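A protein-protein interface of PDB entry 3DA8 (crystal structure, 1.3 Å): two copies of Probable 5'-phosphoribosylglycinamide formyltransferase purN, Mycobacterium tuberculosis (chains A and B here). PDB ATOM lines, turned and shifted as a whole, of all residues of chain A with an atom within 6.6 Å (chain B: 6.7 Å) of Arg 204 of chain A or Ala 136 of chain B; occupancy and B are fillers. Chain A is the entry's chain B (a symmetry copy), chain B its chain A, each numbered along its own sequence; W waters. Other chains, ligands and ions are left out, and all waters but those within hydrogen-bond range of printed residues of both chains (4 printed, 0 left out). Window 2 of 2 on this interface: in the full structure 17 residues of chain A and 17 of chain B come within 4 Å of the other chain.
Gly 138 of chain B touches Ile 158 of chain A (O to CB, 3.7 Å). Arg 204 of chain A touches Ala 136 of chain B. Thr 205 of chain A touches Gly 138 of chain B.
Water W1 lies within hydrogen-bond range of O of Leu 135 of chain B (2.6 Å) and OG1 of Thr 205 of chain A (2.7 Å). Water W3 lies within hydrogen-bond range of OG1 of Thr 205 of chain A (2.7 Å), O of Ala 136 of chain B (3.0 Å) and N of Arg 204 of chain A (3.1 Å). Water W2 lies within hydrogen-bond range of the backbone carbonyl oxygen of Ile 158 of chain A (2.7 Å), the backbone carbonyl oxygen of Gly 138 of chain B (2.8 Å) and the backbone NH of Ala 206 of chain A (2.9 Å). Water W4 lies within hydrogen-bond range of O of Arg 204 of chain A, O of Tyr 137 of chain B and N of Ile 158 of chain A.
No position is printed for both chains. Of the 4 pairs that touch across the chains among the printed residues, none has its exchanged pair printed and touching as well.
The backbone carbonyl oxygen (O) of Tyr 137 of chain B is in hydrogen-bond range of the guanidinium group (NE) of Arg 204 of chain A.
Hydrophobic or aromatic side chains of chain B within 4 Å of the printed part of chain A: Tyr 137. Of the 10 printed residues of chain A, 3 touch a printed residue of chain B. Printed residues of chain A that touch a printed residue of chain B: Ile 158, Arg 204 and Thr 205. Hydrophobic or aromatic side chains of chain A that line the printed part of chain B: Ile 158. Among the printed residues, no Asp or Glu carboxylate lies within 4 Å of a Lys or Arg side-chain nitrogen of the other chain.
The backbone carbonyl oxygen of Gly 156 of chain A lies within hydrogen-bond range of the guanidinium group of Arg 204 of chain A. NH2 of Arg 204 of chain A sits at hydrogen-bond distance from O of Thr 155 of chain A, 2.9 Å away.
Arg 204 of chain A touches just these residues of chain B: Ala 136 and Tyr 137. Ala 136 of chain B touches one residue of chain A. Printed residues of chain A within 4 Å of Tyr 137 of chain B: Arg 204. Printed residues of chain B within 4 Å of Thr 205 of chain A: Gly 138 (3.6 Å). Printed residues of chain A within 4 Å of Gly 138 of chain B: Ile 158 (3.7 Å) and Thr 205 (3.6 Å). Of the printed residues of chain B, Ile 158 of chain A touches Gly 138 (3.7 Å). Val 131 of chain B touches none of the printed residues of chain A. Gly 156 of chain A touches none of the printed residues of chain B. The nearest residue of chain B that does not touch Arg 204 of chain A is Gly 138 of chain B (4.8 Å). The nearest printed residue of chain B that does not touch Thr 205 of chain A is Ala 136 of chain B (4.04 Å).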
ATOM      1  N   THR A 155     -37.861   3.852 -21.625  1.00  0.00           N
ATOM      2  CA  THR A 155     -36.465   4.270 -21.595  1.00  0.00           C
ATOM      3  C   THR A 155     -35.614   3.094 -21.141  1.00  0.00           C
ATOM      4  O   THR A 155     -34.538   3.266 -20.578  1.00  0.00           O
ATOM      5  CB  THR A 155     -36.275   5.458 -20.642  1.00  0.00           C
ATOM      6  OG1 THR A 155     -36.854   5.149 -19.372  1.00  0.00           O
ATOM      7  CG2 THR A 155     -36.937   6.716 -21.207  1.00  0.00           C
ATOM      8  N   GLY A 156     -36.096   1.887 -21.398  1.00  0.00           N
ATOM      9  CA  GLY A 156     -35.389   0.671 -21.008  1.00  0.00           C
ATOM     10  C   GLY A 156     -34.067   0.501 -21.734  1.00  0.00           C
ATOM     11  O   GLY A 156     -33.792   1.182 -22.725  1.00  0.00           O
ATOM     12  N   PRO A 157     -33.225  -0.404 -21.248  1.00  0.00           N
ATOM     13  CA  PRO A 157     -31.907  -0.589 -21.864  1.00  0.00           C
ATOM     14  C   PRO A 157     -31.999  -0.895 -23.358  1.00  0.00           C
ATOM     15  O   PRO A 157     -32.826  -1.696 -23.805  1.00  0.00           O
ATOM     16  CB  PRO A 157     -31.327  -1.768 -21.081  1.00  0.00           C
ATOM     17  CG  PRO A 157     -31.977  -1.651 -19.723  1.00  0.00           C
ATOM     18  CD  PRO A 157     -33.376  -1.185 -20.004  1.00  0.00           C
ATOM     19  N   ILE A 158     -31.150  -0.220 -24.120  1.00  0.00           N
ATOM     20  CA  ILE A 158     -31.102  -0.368 -25.558  1.00  0.00           C
ATOM     21  C   ILE A 158     -30.358  -1.644 -25.963  1.00  0.00           C
ATOM     22  O   ILE A 158     -29.233  -1.886 -25.531  1.00  0.00           O
ATOM     23  CB  ILE A 158     -30.458   0.885 -26.188  1.00  0.00           C
ATOM     24  CG1 ILE A 158     -31.346   2.108 -25.930  1.00  0.00           C
ATOM     25  CG2 ILE A 158     -30.202   0.661 -27.664  1.00  0.00           C
ATOM     26  CD1 ILE A 158     -30.710   3.443 -26.219  1.00  0.00           C
ATOM     27  N   VAL A 201     -27.201  -6.648 -18.245  1.00  0.00           N
ATOM     28  CA  VAL A 201     -27.411  -5.212 -18.098  1.00  0.00           C
ATOM     29  C   VAL A 201     -26.718  -4.719 -16.848  1.00  0.00           C
ATOM     30  O   VAL A 201     -26.997  -5.206 -15.736  1.00  0.00           O
ATOM     31  CB  VAL A 201     -28.901  -4.845 -18.035  1.00  0.00           C
ATOM     32  CG1 VAL A 201     -29.053  -3.332 -17.808  1.00  0.00           C
ATOM     33  CG2 VAL A 201     -29.586  -5.245 -19.326  1.00  0.00           C
ATOM     34  N   VAL A 202     -25.801  -3.773 -17.065  1.00  0.00           N
ATOM     35  CA  VAL A 202     -25.088  -3.055 -16.013  1.00  0.00           C
ATOM     36  C   VAL A 202     -25.364  -1.560 -16.205  1.00  0.00           C
ATOM     37  O   VAL A 202     -25.110  -0.995 -17.283  1.00  0.00           O
ATOM     38  CB  VAL A 202     -23.567  -3.313 -16.079  1.00  0.00           C
ATOM     39  CG1 VAL A 202     -22.854  -2.551 -14.971  1.00  0.00           C
ATOM     40  CG2 VAL A 202     -23.263  -4.806 -15.953  1.00  0.00           C
ATOM     41  N   GLY A 203     -25.888  -0.931 -15.153  1.00  0.00           N
ATOM     42  CA  GLY A 203     -26.362   0.448 -15.232  1.00  0.00           C
ATOM     43  C   GLY A 203     -27.605   0.424 -16.095  1.00  0.00           C
ATOM     44  O   GLY A 203     -28.626  -0.148 -15.707  1.00  0.00           O
ATOM     45  N   ARG A 204     -27.506   1.041 -17.267  1.00  0.00           N
ATOM     46  CA  ARG A 204     -28.554   0.966 -18.283  1.00  0.00           C
ATOM     47  C   ARG A 204     -28.005   0.428 -19.606  1.00  0.00           C
ATOM     48  O   ARG A 204     -28.687   0.484 -20.614  1.00  0.00           O
ATOM     49  CB  ARG A 204     -29.306   2.310 -18.423  1.00  0.00           C
ATOM     50  CG  ARG A 204     -28.445   3.551 -18.751  1.00  0.00           C
ATOM     51  CD  ARG A 204     -29.270   4.747 -19.335  1.00  0.00           C
ATOM     52  NE  ARG A 204     -29.951   4.296 -20.545  1.00  0.00           N
ATOM     53  CZ  ARG A 204     -31.267   4.130 -20.678  1.00  0.00           C
ATOM     54  NH1 ARG A 204     -31.729   3.600 -21.791  1.00  0.00           N
ATOM     55  NH2 ARG A 204     -32.111   4.498 -19.715  1.00  0.00           N
ATOM     56  N   THR A 205     -26.786  -0.112 -19.585  1.00  0.00           N
ATOM     57  CA  THR A 205     -26.127  -0.661 -20.770  1.00  0.00           C
ATOM     58  C   THR A 205     -26.319  -2.154 -20.887  1.00  0.00           C
ATOM     59  O   THR A 205     -25.890  -2.932 -20.023  1.00  0.00           O
ATOM     60  CB  THR A 205     -24.615  -0.370 -20.801  1.00  0.00           C
ATOM     61  OG1 THR A 205     -24.406   1.042 -20.795  1.00  0.00           O
ATOM     62  CG2 THR A 205     -23.970  -0.957 -22.059  1.00  0.00           C
ATOM     63  N   ALA A 206     -26.954  -2.545 -21.978  1.00  0.00           N
ATOM     64  CA  ALA A 206     -27.151  -3.955 -22.268  1.00  0.00           C
ATOM     65  C   ALA A 206     -26.057  -4.438 -23.207  1.00  0.00           C
ATOM     66  O   ALA A 206     -25.799  -3.831 -24.249  1.00  0.00           O
ATOM     67  CB  ALA A 206     -28.518  -4.186 -22.883  1.00  0.00           C
ATOM     68  N   PHE B 125     -27.313  14.185 -27.046  1.00  0.00           N
ATOM     69  CA  PHE B 125     -26.012  14.389 -26.390  1.00  0.00           C
ATOM     70  C   PHE B 125     -25.329  15.708 -26.755  1.00  0.00           C
ATOM     71  O   PHE B 125     -24.179  15.729 -27.211  1.00  0.00           O
ATOM     72  CB  PHE B 125     -25.110  13.170 -26.631  1.00  0.00           C
ATOM     73  CG  PHE B 125     -25.795  11.883 -26.270  1.00  0.00           C
ATOM     74  CD1 PHE B 125     -26.193  11.640 -24.964  1.00  0.00           C
ATOM     75  CD2 PHE B 125     -26.103  10.946 -27.245  1.00  0.00           C
ATOM     76  CE1 PHE B 125     -26.862  10.456 -24.625  1.00  0.00           C
ATOM     77  CE2 PHE B 125     -26.776   9.753 -26.917  1.00  0.00           C
ATOM     78  CZ  PHE B 125     -27.165   9.521 -25.603  1.00  0.00           C
ATOM     79  N   VAL B 131     -19.642  12.534 -26.151  1.00  0.00           N
ATOM     80  CA  VAL B 131     -19.177  11.168 -26.341  1.00  0.00           C
ATOM     81  C   VAL B 131     -19.325  10.345 -25.055  1.00  0.00           C
ATOM     82  O   VAL B 131     -19.891   9.247 -25.071  1.00  0.00           O
ATOM     83  CB  VAL B 131     -17.734  11.131 -26.873  1.00  0.00           C
ATOM     84  CG1 VAL B 131     -17.277   9.699 -27.110  1.00  0.00           C
ATOM     85  CG2 VAL B 131     -17.638  11.961 -28.147  1.00  0.00           C
ATOM     86  N   ALA B 132     -18.837  10.884 -23.941  1.00  0.00           N
ATOM     87  CA  ALA B 132     -18.986  10.211 -22.656  1.00  0.00           C
ATOM     88  C   ALA B 132     -20.443   9.944 -22.300  1.00  0.00           C
ATOM     89  O   ALA B 132     -20.768   8.876 -21.783  1.00  0.00           O
ATOM     90  CB  ALA B 132     -18.303  11.007 -21.546  1.00  0.00           C
ATOM     91  N   ASP B 133     -21.293  10.914 -22.596  1.00  0.00           N
ATOM     92  CA  ASP B 133     -22.707  10.778 -22.284  1.00  0.00           C
ATOM     93  C   ASP B 133     -23.397   9.714 -23.134  1.00  0.00           C
ATOM     94  O   ASP B 133     -24.230   8.974 -22.626  1.00  0.00           O
ATOM     95  CB  ASP B 133     -23.407  12.135 -22.411  1.00  0.00           C
ATOM     96  CG  ASP B 133     -23.001  13.127 -21.304  1.00  0.00           C
ATOM     97  OD1 ASP B 133     -22.353  12.713 -20.315  1.00  0.00           O
ATOM     98  OD2 ASP B 133     -23.345  14.324 -21.412  1.00  0.00           O
ATOM     99  N   ALA B 134     -23.040   9.627 -24.411  1.00  0.00           N
ATOM    100  CA  ALA B 134     -23.606   8.600 -25.287  1.00  0.00           C
ATOM    101  C   ALA B 134     -23.193   7.213 -24.790  1.00  0.00           C
ATOM    102  O   ALA B 134     -24.010   6.295 -24.739  1.00  0.00           O
ATOM    103  CB  ALA B 134     -23.161   8.811 -26.725  1.00  0.00           C
ATOM    104  N   LEU B 135     -21.920   7.078 -24.422  1.00  0.00           N
ATOM    105  CA  LEU B 135     -21.400   5.813 -23.937  1.00  0.00           C
ATOM    106  C   LEU B 135     -22.115   5.404 -22.661  1.00  0.00           C
ATOM    107  O   LEU B 135     -22.557   4.262 -22.529  1.00  0.00           O
ATOM    108  CB  LEU B 135     -19.892   5.928 -23.707  1.00  0.00           C
ATOM    109  CG  LEU B 135     -19.125   4.654 -23.399  1.00  0.00           C
ATOM    110  CD1 LEU B 135     -19.170   3.702 -24.587  1.00  0.00           C
ATOM    111  CD2 LEU B 135     -17.690   5.013 -23.046  1.00  0.00           C
ATOM    112  N   ALA B 136     -22.279   6.340 -21.736  1.00  0.00           N
ATOM    113  CA  ALA B 136     -22.950   6.053 -20.470  1.00  0.00           C
ATOM    114  C   ALA B 136     -24.427   5.703 -20.631  1.00  0.00           C
ATOM    115  O   ALA B 136     -24.962   4.925 -19.847  1.00  0.00           O
ATOM    116  CB  ALA B 136     -22.788   7.210 -19.504  1.00  0.00           C
ATOM    117  N   TYR B 137     -25.083   6.292 -21.628  1.00  0.00           N
ATOM    118  CA  TYR B 137     -26.506   6.035 -21.862  1.00  0.00           C
ATOM    119  C   TYR B 137     -26.711   4.650 -22.460  1.00  0.00           C
ATOM    120  O   TYR B 137     -27.814   4.095 -22.397  1.00  0.00           O
ATOM    121  CB  TYR B 137     -27.111   7.120 -22.771  1.00  0.00           C
ATOM    122  CG  TYR B 137     -28.611   7.143 -22.677  1.00  0.00           C
ATOM    123  CD1 TYR B 137     -29.235   7.849 -21.660  1.00  0.00           C
ATOM    124  CD2 TYR B 137     -29.405   6.437 -23.584  1.00  0.00           C
ATOM    125  CE1 TYR B 137     -30.628   7.856 -21.528  1.00  0.00           C
ATOM    126  CE2 TYR B 137     -30.799   6.425 -23.453  1.00  0.00           C
ATOM    127  CZ  TYR B 137     -31.396   7.140 -22.431  1.00  0.00           C
ATOM    128  OH  TYR B 137     -32.765   7.132 -22.285  1.00  0.00           O
ATOM    129  N   GLY B 138     -25.682   4.090 -23.078  1.00  0.00           N
ATOM    130  CA  GLY B 138     -25.758   2.769 -23.666  1.00  0.00           C
ATOM    131  C   GLY B 138     -26.367   2.728 -25.049  1.00  0.00           C
ATOM    132  O   GLY B 138     -26.915   1.702 -25.451  1.00  0.00           O
ATOM    133  N   VAL B 139     -26.259   3.827 -25.797  1.00  0.00           N
ATOM    134  CA  VAL B 139     -26.697   3.777 -27.191  1.00  0.00           C
ATOM    135  C   VAL B 139     -25.772   2.859 -27.997  1.00  0.00           C
ATOM    136  O   VAL B 139     -24.609   2.622 -27.623  1.00  0.00           O
ATOM    137  CB  VAL B 139     -26.768   5.175 -27.854  1.00  0.00           C
ATOM    138  CG1 VAL B 139     -27.754   6.064 -27.108  1.00  0.00           C
ATOM    139  CG2 VAL B 139     -25.382   5.854 -27.973  1.00  0.00           C
HETATM  140  O   HOH W   1     -22.017   1.820 -21.851  1.00  0.00           O
HETATM  141  O   HOH W   2     -27.460  -0.601 -24.003  1.00  0.00           O
HETATM  142  O   HOH W   3     -24.950   2.286 -18.503  1.00  0.00           O
HETATM  143  O   HOH W   4     -29.534   1.878 -22.747  1.00  0.00           O
